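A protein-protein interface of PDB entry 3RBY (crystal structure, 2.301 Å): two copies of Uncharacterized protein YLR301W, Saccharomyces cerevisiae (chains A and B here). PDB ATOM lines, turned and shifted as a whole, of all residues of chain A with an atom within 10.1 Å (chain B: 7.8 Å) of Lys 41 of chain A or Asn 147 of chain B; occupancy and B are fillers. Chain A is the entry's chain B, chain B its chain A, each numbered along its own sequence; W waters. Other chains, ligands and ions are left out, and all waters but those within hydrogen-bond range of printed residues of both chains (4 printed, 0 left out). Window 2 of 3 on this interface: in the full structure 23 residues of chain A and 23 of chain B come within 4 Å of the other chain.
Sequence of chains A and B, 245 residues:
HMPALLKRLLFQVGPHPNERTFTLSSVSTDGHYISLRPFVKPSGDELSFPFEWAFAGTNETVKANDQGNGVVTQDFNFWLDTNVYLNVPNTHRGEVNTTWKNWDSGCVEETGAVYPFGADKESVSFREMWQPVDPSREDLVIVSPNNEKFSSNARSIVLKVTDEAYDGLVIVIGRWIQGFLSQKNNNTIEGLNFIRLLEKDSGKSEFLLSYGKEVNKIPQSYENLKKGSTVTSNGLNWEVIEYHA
N of Ser 105 of chain B is in hydrogen-bond range of O of Glu 19 of chain A (3.3 Å). ND2 of Asn 147 of chain B lies close to NZ of Lys 41 of chain A (3.5 Å).
The backbone NH (N) of Asn 146 of chain B sits at hydrogen-bond distance from the side-chain carboxylate (OE1) of Glu 148 of chain B. The side-chain carboxylate (OE1) of Glu 19 of chain A sits at hydrogen-bond distance from the side-chain hydroxyl (OG1) of Thr 21 of chain A (2.5 Å). The backbone NH (N) of Val 40 of chain A is in hydrogen-bond range of the backbone carbonyl oxygen (O) of Arg 20 of chain A, 2.8 Å away. OE2 of Glu 46 of chain A lies within salt-bridge range of NH1 of Arg 20 of chain A (2.8 Å). N of Phe 22 of chain A lies within hydrogen-bond range of O of Pro 38 of chain A, at 3.0 Å.
Among the printed residues, pairs that only touch across the chains: Asn 18 of chain A with Trp 103 of chain B, Glu 19 of chain A with Trp 103 of chain B, Glu 19 of chain A with Asp 104 of chain B, Arg 20 of chain A with Asp 104 of chain B, Phe 22 of chain A with Asn 146 of chain B, Val 40 of chain A with Asp 104 of chain B, Val 40 of chain A with Pro 145 of chain B, Val 40 of chain A with Asn 146 of chain B, Val 40 of chain A with Asn 147 of chain B, Lys 41 of chain A with Asp 104 of chain B and Leu 140 of chain A with Pro 145 of chain B.
Of the printed residues of chain B, Glu 19 of chain A touches Trp 103, Asp 104 and Ser 105. Of the printed residues of chain B, Val 40 of chain A touches Asp 104, Pro 145, Asn 146 and Asn 147. Of chain B, only Asp 104 (3.6 Å) and Asn 147 (3.3 Å) come within 4 Å of Lys 41 of chain A. Of chain A, only Glu 19, Arg 20, Val 40 and Lys 41 come within 4 Å of Asp 104 of chain B. Of the printed residues of chain A, Ser 105 of chain B touches Glu 19 (3.3 Å). Asn 146 of chain B touches just these residues of chain A: Phe 22 (3.7 Å) and Val 40 (3.3 Å). Of the printed residues of chain A, Asn 147 of chain B touches Val 40 and Lys 41. Glu 148 of chain B touches none of the printed residues of chain A. The nearest residue of chain A that does not touch Asn 147 of chain B is Phe 22 of chain A (7.1 Å). The nearest printed residue of chain A that does not touch Trp 103 of chain B is Lys 41 of chain A (5.9 Å).
Of the 22 printed residues of chain A, 7 touch a printed residue of chain B. Printed residues of chain B that touch a printed residue of chain A: Trp 103, Asp 104, Ser 105, Pro 145, Asn 146 and Asn 147. Hydrophobic or aromatic side chains of chain B within 4 Å of the printed part of chain A: Trp 103 and Pro 145. Among the printed residues, no Asp or Glu carboxylate lies within 4 Å of a Lys or Arg side-chain nitrogen of the other chain.
No position is printed for both chains. Of the 13 pairs that touch across the chains among the printed residues, none has its exchanged pair printed and touching as well.
Water W2 lies within hydrogen-bond range of the backbone carbonyl oxygen of Thr 21 of chain A (2.6 Å), the side-chain amino group of Lys 7 of chain A (2.8 Å) and the backbone carbonyl oxygen of Pro 145 of chain B (2.9 Å). Water W1 bridges N of Asp 104 of chain B (2.7 Å) and OD1 of Asn 18 of chain A (2.8 Å). Water W4 lies within hydrogen-bond range of OD1 of Asn 146 of chain B (2.8 Å) and O of Phe 39 of chain A (2.9 Å).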
ATOM      1  N   LYS A   7       0.422 -30.051   2.321  1.00  0.00           N
ATOM      2  CA  LYS A   7      -0.345 -29.358   3.340  1.00  0.00           C
ATOM      3  C   LYS A   7      -1.530 -30.231   3.741  1.00  0.00           C
ATOM      4  O   LYS A   7      -2.306 -30.675   2.885  1.00  0.00           O
ATOM      5  CB  LYS A   7      -0.801 -27.996   2.828  1.00  0.00           C
ATOM      6  CG  LYS A   7      -1.262 -27.027   3.936  1.00  0.00           C
ATOM      7  CD  LYS A   7      -2.755 -27.202   4.229  1.00  0.00           C
ATOM      8  CE  LYS A   7      -3.273 -26.190   5.241  1.00  0.00           C
ATOM      9  NZ  LYS A   7      -4.675 -26.551   5.614  1.00  0.00           N
ATOM     10  N   ASN A  18     -11.686 -33.337  11.080  1.00  0.00           N
ATOM     11  CA  ASN A  18     -11.487 -31.948  11.477  1.00  0.00           C
ATOM     12  C   ASN A  18     -10.054 -31.554  11.116  1.00  0.00           C
ATOM     13  O   ASN A  18      -9.278 -32.393  10.662  1.00  0.00           O
ATOM     14  CB  ASN A  18     -11.745 -31.812  12.978  1.00  0.00           C
ATOM     15  CG  ASN A  18     -11.784 -30.360  13.458  1.00  0.00           C
ATOM     16  OD1 ASN A  18     -11.938 -29.420  12.671  1.00  0.00           O
ATOM     17  ND2 ASN A  18     -11.646 -30.179  14.774  1.00  0.00           N
ATOM     18  N   GLU A  19      -9.691 -30.290  11.299  1.00  0.00           N
ATOM     19  CA  GLU A  19      -8.309 -29.878  11.045  1.00  0.00           C
ATOM     20  C   GLU A  19      -7.901 -28.695  11.916  1.00  0.00           C
ATOM     21  O   GLU A  19      -8.221 -27.534  11.627  1.00  0.00           O
ATOM     22  CB  GLU A  19      -8.058 -29.584   9.555  1.00  0.00           C
ATOM     23  CG  GLU A  19      -6.612 -29.227   9.251  1.00  0.00           C
ATOM     24  CD  GLU A  19      -5.646 -30.318   9.708  1.00  0.00           C
ATOM     25  OE1 GLU A  19      -5.151 -30.246  10.861  1.00  0.00           O
ATOM     26  OE2 GLU A  19      -5.396 -31.256   8.910  1.00  0.00           O
ATOM     27  N   ARG A  20      -7.159 -29.008  12.970  1.00  0.00           N
ATOM     28  CA  ARG A  20      -6.780 -28.016  13.957  1.00  0.00           C
ATOM     29  C   ARG A  20      -5.365 -27.491  13.707  1.00  0.00           C
ATOM     30  O   ARG A  20      -4.868 -26.618  14.442  1.00  0.00           O
ATOM     31  CB  ARG A  20      -6.881 -28.635  15.361  1.00  0.00           C
ATOM     32  CG  ARG A  20      -8.282 -29.124  15.719  1.00  0.00           C
ATOM     33  CD  ARG A  20      -8.744 -28.571  17.073  1.00  0.00           C
ATOM     34  NE  ARG A  20      -8.033 -29.210  18.170  1.00  0.00           N
ATOM     35  CZ  ARG A  20      -7.330 -28.567  19.097  1.00  0.00           C
ATOM     36  NH1 ARG A  20      -6.707 -29.260  20.044  1.00  0.00           N
ATOM     37  NH2 ARG A  20      -7.247 -27.241  19.087  1.00  0.00           N
ATOM     38  N   THR A  21      -4.717 -28.010  12.667  1.00  0.00           N
ATOM     39  CA  THR A  21      -3.312 -27.689  12.442  1.00  0.00           C
ATOM     40  C   THR A  21      -3.064 -26.888  11.161  1.00  0.00           C
ATOM     41  O   THR A  21      -3.877 -26.907  10.234  1.00  0.00           O
ATOM     42  CB  THR A  21      -2.442 -28.965  12.423  1.00  0.00           C
ATOM     43  OG1 THR A  21      -2.704 -29.721  11.233  1.00  0.00           O
ATOM     44  CG2 THR A  21      -2.729 -29.848  13.661  1.00  0.00           C
ATOM     45  N   PHE A  22      -1.956 -26.150  11.143  1.00  0.00           N
ATOM     46  CA  PHE A  22      -1.317 -25.769   9.894  1.00  0.00           C
ATOM     47  C   PHE A  22      -0.138 -26.750   9.690  1.00  0.00           C
ATOM     48  O   PHE A  22       1.017 -26.437   9.981  1.00  0.00           O
ATOM     49  CB  PHE A  22      -0.832 -24.322   9.929  1.00  0.00           C
ATOM     50  CG  PHE A  22      -0.166 -23.868   8.654  1.00  0.00           C
ATOM     51  CD1 PHE A  22       0.496 -22.642   8.609  1.00  0.00           C
ATOM     52  CD2 PHE A  22      -0.203 -24.655   7.499  1.00  0.00           C
ATOM     53  CE1 PHE A  22       1.119 -22.206   7.443  1.00  0.00           C
ATOM     54  CE2 PHE A  22       0.413 -24.231   6.322  1.00  0.00           C
ATOM     55  CZ  PHE A  22       1.072 -23.001   6.295  1.00  0.00           C
ATOM     56  N   ARG A  37       3.313 -30.008  13.009  1.00  0.00           N
ATOM     57  CA  ARG A  37       1.863 -29.862  13.052  1.00  0.00           C
ATOM     58  C   ARG A  37       1.409 -28.931  14.182  1.00  0.00           C
ATOM     59  O   ARG A  37       0.817 -29.378  15.169  1.00  0.00           O
ATOM     60  CB  ARG A  37       1.229 -31.262  13.132  1.00  0.00           C
ATOM     61  CG  ARG A  37       1.476 -32.041  11.826  1.00  0.00           C
ATOM     62  CD  ARG A  37       2.084 -33.434  11.958  1.00  0.00           C
ATOM     63  NE  ARG A  37       1.074 -34.478  11.824  1.00  0.00           N
ATOM     64  CZ  ARG A  37       1.007 -35.388  10.848  1.00  0.00           C
ATOM     65  NH1 ARG A  37       1.897 -35.426   9.862  1.00  0.00           N
ATOM     66  NH2 ARG A  37       0.024 -36.281  10.871  1.00  0.00           N
ATOM     67  N   PRO A  38       1.686 -27.623  14.041  1.00  0.00           N
ATOM     68  CA  PRO A  38       1.228 -26.661  15.051  1.00  0.00           C
ATOM     69  C   PRO A  38      -0.289 -26.466  15.012  1.00  0.00           C
ATOM     70  O   PRO A  38      -0.893 -26.544  13.928  1.00  0.00           O
ATOM     71  CB  PRO A  38       1.917 -25.356  14.630  1.00  0.00           C
ATOM     72  CG  PRO A  38       2.098 -25.498  13.137  1.00  0.00           C
ATOM     73  CD  PRO A  38       2.379 -26.971  12.915  1.00  0.00           C
ATOM     74  N   PHE A  39      -0.896 -26.209  16.170  1.00  0.00           N
ATOM     75  CA  PHE A  39      -2.315 -25.871  16.206  1.00  0.00           C
ATOM     76  C   PHE A  39      -2.495 -24.465  15.705  1.00  0.00           C
ATOM     77  O   PHE A  39      -1.633 -23.601  15.919  1.00  0.00           O
ATOM     78  CB  PHE A  39      -2.874 -25.937  17.630  1.00  0.00           C
ATOM     79  CG  PHE A  39      -2.930 -27.329  18.206  1.00  0.00           C
ATOM     80  CD1 PHE A  39      -2.196 -27.656  19.345  1.00  0.00           C
ATOM     81  CD2 PHE A  39      -3.720 -28.303  17.622  1.00  0.00           C
ATOM     82  CE1 PHE A  39      -2.247 -28.939  19.892  1.00  0.00           C
ATOM     83  CE2 PHE A  39      -3.783 -29.596  18.162  1.00  0.00           C
ATOM     84  CZ  PHE A  39      -3.040 -29.911  19.302  1.00  0.00           C
ATOM     85  N   VAL A  40      -3.627 -24.219  15.059  1.00  0.00           N
ATOM     86  CA  VAL A  40      -3.971 -22.858  14.675  1.00  0.00           C
ATOM     87  C   VAL A  40      -4.495 -22.086  15.888  1.00  0.00           C
ATOM     88  O   VAL A  40      -4.066 -20.964  16.134  1.00  0.00           O
ATOM     89  CB  VAL A  40      -5.013 -22.831  13.558  1.00  0.00           C
ATOM     90  CG1 VAL A  40      -5.378 -21.378  13.207  1.00  0.00           C
ATOM     91  CG2 VAL A  40      -4.481 -23.588  12.334  1.00  0.00           C
ATOM     92  N   LYS A  41      -5.429 -22.697  16.622  1.00  0.00           N
ATOM     93  CA  LYS A  41      -6.021 -22.092  17.818  1.00  0.00           C
ATOM     94  C   LYS A  41      -5.895 -23.062  18.989  1.00  0.00           C
ATOM     95  O   LYS A  41      -6.861 -23.753  19.353  1.00  0.00           O
ATOM     96  CB  LYS A  41      -7.499 -21.739  17.597  1.00  0.00           C
ATOM     97  CG  LYS A  41      -7.762 -20.833  16.397  1.00  0.00           C
ATOM     98  CD  LYS A  41      -9.251 -20.448  16.307  1.00  0.00           C
ATOM     99  CE  LYS A  41      -9.660 -20.134  14.857  1.00  0.00           C
ATOM    100  NZ  LYS A  41     -10.900 -19.289  14.753  1.00  0.00           N
ATOM    101  N   PRO A  42      -4.690 -23.131  19.573  1.00  0.00           N
ATOM    102  CA  PRO A  42      -4.451 -24.013  20.724  1.00  0.00           C
ATOM    103  C   PRO A  42      -5.312 -23.562  21.908  1.00  0.00           C
ATOM    104  O   PRO A  42      -5.573 -22.355  22.037  1.00  0.00           O
ATOM    105  CB  PRO A  42      -2.960 -23.790  21.030  1.00  0.00           C
ATOM    106  CG  PRO A  42      -2.655 -22.401  20.483  1.00  0.00           C
ATOM    107  CD  PRO A  42      -3.527 -22.275  19.258  1.00  0.00           C
ATOM    108  N   SER A  43      -5.767 -24.509  22.729  1.00  0.00           N
ATOM    109  CA  SER A  43      -6.482 -24.185  23.968  1.00  0.00           C
ATOM    110  C   SER A  43      -5.473 -23.771  25.038  1.00  0.00           C
ATOM    111  O   SER A  43      -4.260 -23.881  24.823  1.00  0.00           O
ATOM    112  CB  SER A  43      -7.262 -25.401  24.465  1.00  0.00           C
ATOM    113  OG  SER A  43      -6.383 -26.352  25.043  1.00  0.00           O
ATOM    114  N   GLY A  44      -5.960 -23.296  26.185  1.00  0.00           N
ATOM    115  CA  GLY A  44      -5.076 -22.942  27.286  1.00  0.00           C
ATOM    116  C   GLY A  44      -4.155 -24.092  27.669  1.00  0.00           C
ATOM    117  O   GLY A  44      -2.959 -23.908  27.938  1.00  0.00           O
ATOM    118  N   ASP A  45      -4.719 -25.292  27.681  1.00  0.00           N
ATOM    119  CA  ASP A  45      -3.978 -26.498  28.038  1.00  0.00           C
ATOM    120  C   ASP A  45      -2.786 -26.767  27.106  1.00  0.00           C
ATOM    121  O   ASP A  45      -1.731 -27.253  27.538  1.00  0.00           O
ATOM    122  CB  ASP A  45      -4.936 -27.693  28.037  1.00  0.00           C
ATOM    123  CG  ASP A  45      -6.230 -27.398  28.792  1.00  0.00           C
ATOM    124  OD1 ASP A  45      -7.068 -26.614  28.271  1.00  0.00           O
ATOM    125  OD2 ASP A  45      -6.400 -27.944  29.909  1.00  0.00           O
ATOM    126  N   GLU A  46      -2.958 -26.437  25.827  1.00  0.00           N
ATOM    127  CA  GLU A  46      -1.949 -26.727  24.812  1.00  0.00           C
ATOM    128  C   GLU A  46      -1.107 -25.493  24.468  1.00  0.00           C
ATOM    129  O   GLU A  46      -0.285 -25.528  23.549  1.00  0.00           O
ATOM    130  CB  GLU A  46      -2.596 -27.362  23.563  1.00  0.00           C
ATOM    131  CG  GLU A  46      -3.974 -26.822  23.235  1.00  0.00           C
ATOM    132  CD  GLU A  46      -4.786 -27.695  22.267  1.00  0.00           C
ATOM    133  OE1 GLU A  46      -4.763 -28.944  22.371  1.00  0.00           O
ATOM    134  OE2 GLU A  46      -5.478 -27.106  21.405  1.00  0.00           O
ATOM    135  N   LEU A  47      -1.292 -24.417  25.232  1.00  0.00           N
ATOM    136  CA  LEU A  47      -0.516 -23.192  25.041  1.00  0.00           C
ATOM    137  C   LEU A  47       0.976 -23.443  25.158  1.00  0.00           C
ATOM    138  O   LEU A  47       1.753 -22.923  24.373  1.00  0.00           O
ATOM    139  CB  LEU A  47      -0.937 -22.132  26.053  1.00  0.00           C
ATOM    140  CG  LEU A  47      -1.685 -20.920  25.493  1.00  0.00           C
ATOM    141  CD1 LEU A  47      -2.376 -21.282  24.191  1.00  0.00           C
ATOM    142  CD2 LEU A  47      -2.684 -20.343  26.505  1.00  0.00           C
ATOM    143  N   PHE A  49       2.705 -26.054  24.529  1.00  0.00           N
ATOM    144  CA  PHE A  49       3.246 -26.917  23.483  1.00  0.00           C
ATOM    145  C   PHE A  49       2.221 -27.040  22.382  1.00  0.00           C
ATOM    146  O   PHE A  49       1.534 -28.059  22.269  1.00  0.00           O
ATOM    147  CB  PHE A  49       3.593 -28.292  24.046  1.00  0.00           C
ATOM    148  CG  PHE A  49       4.235 -29.203  23.053  1.00  0.00           C
ATOM    149  CD1 PHE A  49       5.544 -28.995  22.651  1.00  0.00           C
ATOM    150  CD2 PHE A  49       3.535 -30.279  22.522  1.00  0.00           C
ATOM    151  CE1 PHE A  49       6.150 -29.851  21.738  1.00  0.00           C
ATOM    152  CE2 PHE A  49       4.128 -31.135  21.608  1.00  0.00           C
ATOM    153  CZ  PHE A  49       5.440 -30.919  21.216  1.00  0.00           C
ATOM    154  N   PRO A  50       2.122 -25.983  21.567  1.00  0.00           N
ATOM    155  CA  PRO A  50       1.049 -25.775  20.588  1.00  0.00           C
ATOM    156  C   PRO A  50       1.192 -26.597  19.303  1.00  0.00           C
ATOM    157  O   PRO A  50       1.149 -26.032  18.202  1.00  0.00           O
ATOM    158  CB  PRO A  50       1.131 -24.269  20.298  1.00  0.00           C
ATOM    159  CG  PRO A  50       2.538 -23.887  20.576  1.00  0.00           C
ATOM    160  CD  PRO A  50       3.084 -24.865  21.598  1.00  0.00           C
ATOM    161  N   PHE A  51       1.361 -27.908  19.445  1.00  0.00           N
ATOM    162  CA  PHE A  51       1.511 -28.789  18.294  1.00  0.00           C
ATOM    163  C   PHE A  51       0.776 -30.108  18.506  1.00  0.00           C
ATOM    164  O   PHE A  51       0.932 -30.757  19.541  1.00  0.00           O
ATOM    165  CB  PHE A  51       2.991 -29.052  18.010  1.00  0.00           C
ATOM    166  CG  PHE A  51       3.820 -27.804  17.908  1.00  0.00           C
ATOM    167  CD1 PHE A  51       4.319 -27.192  19.045  1.00  0.00           C
ATOM    168  CD2 PHE A  51       4.100 -27.241  16.674  1.00  0.00           C
ATOM    169  CE1 PHE A  51       5.082 -26.043  18.954  1.00  0.00           C
ATOM    170  CE2 PHE A  51       4.862 -26.093  16.575  1.00  0.00           C
ATOM    171  CZ  PHE A  51       5.354 -25.493  17.718  1.00  0.00           C
ATOM    172  N   GLU A  52      -0.031 -30.493  17.526  1.00  0.00           N
ATOM    173  CA  GLU A  52      -0.778 -31.739  17.604  1.00  0.00           C
ATOM    174  C   GLU A  52       0.296 -32.808  17.749  1.00  0.00           C
ATOM    175  O   GLU A  52       0.209 -33.679  18.612  1.00  0.00           O
ATOM    176  CB  GLU A  52      -1.799 -31.817  16.469  1.00  0.00           C
ATOM    177  CG  GLU A  52      -2.571 -33.122  16.416  1.00  0.00           C
ATOM    178  CD  GLU A  52      -3.509 -33.194  15.229  1.00  0.00           C
ATOM    179  OE1 GLU A  52      -4.639 -32.673  15.331  1.00  0.00           O
ATOM    180  OE2 GLU A  52      -3.114 -33.767  14.193  1.00  0.00           O
ATOM    181  N   LEU A 140       0.901 -20.567  -0.494  1.00  0.00           N
ATOM    182  CA  LEU A 140       0.426 -21.940  -0.668  1.00  0.00           C
ATOM    183  C   LEU A 140      -0.372 -22.044  -1.983  1.00  0.00           C
ATOM    184  O   LEU A 140      -1.549 -21.648  -2.066  1.00  0.00           O
ATOM    185  CB  LEU A 140      -0.463 -22.365   0.512  1.00  0.00           C
ATOM    186  CG  LEU A 140       0.234 -22.577   1.852  1.00  0.00           C
ATOM    187  CD1 LEU A 140      -0.810 -22.832   2.905  1.00  0.00           C
ATOM    188  CD2 LEU A 140       1.208 -23.749   1.780  1.00  0.00           C
ATOM    189  N   ASN B 102     -17.071 -23.807   9.423  1.00  0.00           N
ATOM    190  CA  ASN B 102     -15.678 -23.381   9.291  1.00  0.00           C
ATOM    191  C   ASN B 102     -14.749 -24.176  10.209  1.00  0.00           C
ATOM    192  O   ASN B 102     -15.059 -24.363  11.393  1.00  0.00           O
ATOM    193  CB  ASN B 102     -15.521 -21.885   9.614  1.00  0.00           C
ATOM    194  CG  ASN B 102     -16.170 -20.979   8.574  1.00  0.00           C
ATOM    195  OD1 ASN B 102     -16.222 -21.304   7.383  1.00  0.00           O
ATOM    196  ND2 ASN B 102     -16.663 -19.829   9.023  1.00  0.00           N
ATOM    197  N   TRP B 103     -13.619 -24.650   9.679  1.00  0.00           N
ATOM    198  CA  TRP B 103     -12.601 -25.270  10.538  1.00  0.00           C
ATOM    199  C   TRP B 103     -11.491 -24.285  10.840  1.00  0.00           C
ATOM    200  O   TRP B 103     -11.333 -23.288  10.130  1.00  0.00           O
ATOM    201  CB  TRP B 103     -12.000 -26.502   9.877  1.00  0.00           C
ATOM    202  CG  TRP B 103     -12.931 -27.637   9.785  1.00  0.00           C
ATOM    203  CD1 TRP B 103     -14.206 -27.684  10.253  1.00  0.00           C
ATOM    204  CD2 TRP B 103     -12.677 -28.912   9.167  1.00  0.00           C
ATOM    205  NE1 TRP B 103     -14.766 -28.912   9.974  1.00  0.00           N
ATOM    206  CE2 TRP B 103     -13.847 -29.683   9.308  1.00  0.00           C
ATOM    207  CE3 TRP B 103     -11.574 -29.472   8.512  1.00  0.00           C
ATOM    208  CZ2 TRP B 103     -13.949 -30.990   8.813  1.00  0.00           C
ATOM    209  CZ3 TRP B 103     -11.673 -30.772   8.027  1.00  0.00           C
ATOM    210  CH2 TRP B 103     -12.851 -31.516   8.181  1.00  0.00           C
ATOM    211  N   ASP B 104     -10.710 -24.564  11.880  1.00  0.00           N
ATOM    212  CA  ASP B 104      -9.560 -23.715  12.195  1.00  0.00           C
ATOM    213  C   ASP B 104      -8.595 -23.600  11.003  1.00  0.00           C
ATOM    214  O   ASP B 104      -7.895 -22.595  10.854  1.00  0.00           O
ATOM    215  CB  ASP B 104      -8.803 -24.266  13.407  1.00  0.00           C
ATOM    216  CG  ASP B 104      -9.629 -24.243  14.689  1.00  0.00           C
ATOM    217  OD1 ASP B 104      -9.204 -24.910  15.658  1.00  0.00           O
ATOM    218  OD2 ASP B 104     -10.686 -23.572  14.735  1.00  0.00           O
ATOM    219  N   SER B 105      -8.548 -24.636  10.164  1.00  0.00           N
ATOM    220  CA  SER B 105      -7.621 -24.632   9.028  1.00  0.00           C
ATOM    221  C   SER B 105      -8.037 -23.637   7.952  1.00  0.00           C
ATOM    222  O   SER B 105      -7.275 -23.383   7.020  1.00  0.00           O
ATOM    223  CB  SER B 105      -7.539 -26.011   8.405  1.00  0.00           C
ATOM    224  OG  SER B 105      -8.813 -26.372   7.904  1.00  0.00           O
ATOM    225  N   GLY B 106      -9.245 -23.082   8.082  1.00  0.00           N
ATOM    226  CA  GLY B 106      -9.755 -22.117   7.118  1.00  0.00           C
ATOM    227  C   GLY B 106     -10.490 -22.770   5.953  1.00  0.00           C
ATOM    228  O   GLY B 106     -10.998 -22.069   5.065  1.00  0.00           O
ATOM    229  N   VAL B 143      -6.259 -19.688   0.989  1.00  0.00           N
ATOM    230  CA  VAL B 143      -6.465 -18.473   1.770  1.00  0.00           C
ATOM    231  C   VAL B 143      -6.516 -18.850   3.245  1.00  0.00           C
ATOM    232  O   VAL B 143      -7.160 -19.842   3.597  1.00  0.00           O
ATOM    233  CB  VAL B 143      -7.807 -17.809   1.366  1.00  0.00           C
ATOM    234  CG1 VAL B 143      -8.506 -17.165   2.563  1.00  0.00           C
ATOM    235  CG2 VAL B 143      -7.605 -16.809   0.236  1.00  0.00           C
ATOM    236  N   SER B 144      -5.843 -18.085   4.105  1.00  0.00           N
ATOM    237  CA  SER B 144      -5.953 -18.284   5.558  1.00  0.00           C
ATOM    238  C   SER B 144      -5.753 -19.729   6.044  1.00  0.00           C
ATOM    239  O   SER B 144      -6.663 -20.306   6.655  1.00  0.00           O
ATOM    240  CB  SER B 144      -7.327 -17.804   6.063  1.00  0.00           C
ATOM    241  OG  SER B 144      -7.557 -16.448   5.730  1.00  0.00           O
ATOM    242  N   PRO B 145      -4.569 -20.318   5.796  1.00  0.00           N
ATOM    243  CA  PRO B 145      -4.307 -21.653   6.358  1.00  0.00           C
ATOM    244  C   PRO B 145      -4.142 -21.585   7.870  1.00  0.00           C
ATOM    245  O   PRO B 145      -4.263 -22.608   8.551  1.00  0.00           O
ATOM    246  CB  PRO B 145      -2.964 -22.032   5.730  1.00  0.00           C
ATOM    247  CG  PRO B 145      -2.288 -20.697   5.440  1.00  0.00           C
ATOM    248  CD  PRO B 145      -3.420 -19.800   5.022  1.00  0.00           C
ATOM    249  N   ASN B 146      -3.807 -20.403   8.382  1.00  0.00           N
ATOM    250  CA  ASN B 146      -3.466 -20.247   9.793  1.00  0.00           C
ATOM    251  C   ASN B 146      -4.051 -18.993  10.440  1.00  0.00           C
ATOM    252  O   ASN B 146      -3.321 -18.136  10.937  1.00  0.00           O
ATOM    253  CB  ASN B 146      -1.947 -20.268   9.979  1.00  0.00           C
ATOM    254  CG  ASN B 146      -1.539 -20.389  11.434  1.00  0.00           C
ATOM    255  OD1 ASN B 146      -2.224 -21.027  12.232  1.00  0.00           O
ATOM    256  ND2 ASN B 146      -0.416 -19.774  11.787  1.00  0.00           N
ATOM    257  N   ASN B 147      -5.375 -18.897  10.417  1.00  0.00           N
ATOM    258  CA  ASN B 147      -6.088 -17.812  11.082  1.00  0.00           C
ATOM    259  C   ASN B 147      -5.769 -16.407  10.570  1.00  0.00           C
ATOM    260  O   ASN B 147      -6.083 -15.422  11.239  1.00  0.00           O
ATOM    261  CB  ASN B 147      -5.860 -17.876  12.595  1.00  0.00           C
ATOM    262  CG  ASN B 147      -6.961 -17.191  13.380  1.00  0.00           C
ATOM    263  OD1 ASN B 147      -6.714 -16.226  14.103  1.00  0.00           O
ATOM    264  ND2 ASN B 147      -8.184 -17.689  13.241  1.00  0.00           N
ATOM    265  N   GLU B 148      -5.155 -16.305   9.395  1.00  0.00           N
ATOM    266  CA  GLU B 148      -4.879 -14.985   8.830  1.00  0.00           C
ATOM    267  C   GLU B 148      -6.171 -14.245   8.476  1.00  0.00           C
ATOM    268  O   GLU B 148      -7.184 -14.872   8.152  1.00  0.00           O
ATOM    269  CB  GLU B 148      -4.010 -15.074   7.566  1.00  0.00           C
ATOM    270  CG  GLU B 148      -2.630 -15.653   7.768  1.00  0.00           C
ATOM    271  CD  GLU B 148      -2.614 -17.170   7.657  1.00  0.00           C
ATOM    272  OE1 GLU B 148      -3.688 -17.816   7.682  1.00  0.00           O
ATOM    273  OE2 GLU B 148      -1.516 -17.721   7.537  1.00  0.00           O
ATOM    274  N   LYS B 149      -6.124 -12.916   8.550  1.00  0.00           N
ATOM    275  CA  LYS B 149      -7.149 -12.052   7.962  1.00  0.00           C
ATOM    276  C   LYS B 149      -7.025 -12.090   6.437  1.00  0.00           C
ATOM    277  O   LYS B 149      -5.930 -11.938   5.891  1.00  0.00           O
ATOM    278  CB  LYS B 149      -6.979 -10.594   8.433  1.00  0.00           C
ATOM    279  CG  LYS B 149      -5.821 -10.364   9.418  1.00  0.00           C
ATOM    280  CD  LYS B 149      -4.456 -10.672   8.788  1.00  0.00           C
ATOM    281  CE  LYS B 149      -3.519 -11.342   9.806  1.00  0.00           C
ATOM    282  NZ  LYS B 149      -2.265 -11.881   9.175  1.00  0.00           N
ATOM    283  N   PHE B 150      -8.131 -12.314   5.740  1.00  0.00           N
ATOM    284  CA  PHE B 150      -8.085 -12.237   4.285  1.00  0.00           C
ATOM    285  C   PHE B 150      -9.064 -11.205   3.761  1.00  0.00           C
ATOM    286  O   PHE B 150     -10.256 -11.243   4.076  1.00  0.00           O
ATOM    287  CB  PHE B 150      -8.376 -13.585   3.633  1.00  0.00           C
ATOM    288  CG  PHE B 150      -8.370 -13.531   2.135  1.00  0.00           C
ATOM    289  CD1 PHE B 150      -9.557 -13.608   1.421  1.00  0.00           C
ATOM    290  CD2 PHE B 150      -7.179 -13.370   1.436  1.00  0.00           C
ATOM    291  CE1 PHE B 150      -9.562 -13.536   0.030  1.00  0.00           C
ATOM    292  CE2 PHE B 150      -7.174 -13.297   0.039  1.00  0.00           C
ATOM    293  CZ  PHE B 150      -8.367 -13.378  -0.664  1.00  0.00           C
HETATM  294  O   HOH W   1     -11.350 -26.734  13.383  1.00  0.00           O
HETATM  295  O   HOH W   2      -4.279 -25.489   8.134  1.00  0.00           O
HETATM  296  O   HOH W   3      -6.550 -25.374  16.445  1.00  0.00           O
HETATM  297  O   HOH W   4      -0.328 -22.615  13.565  1.00  0.00           O
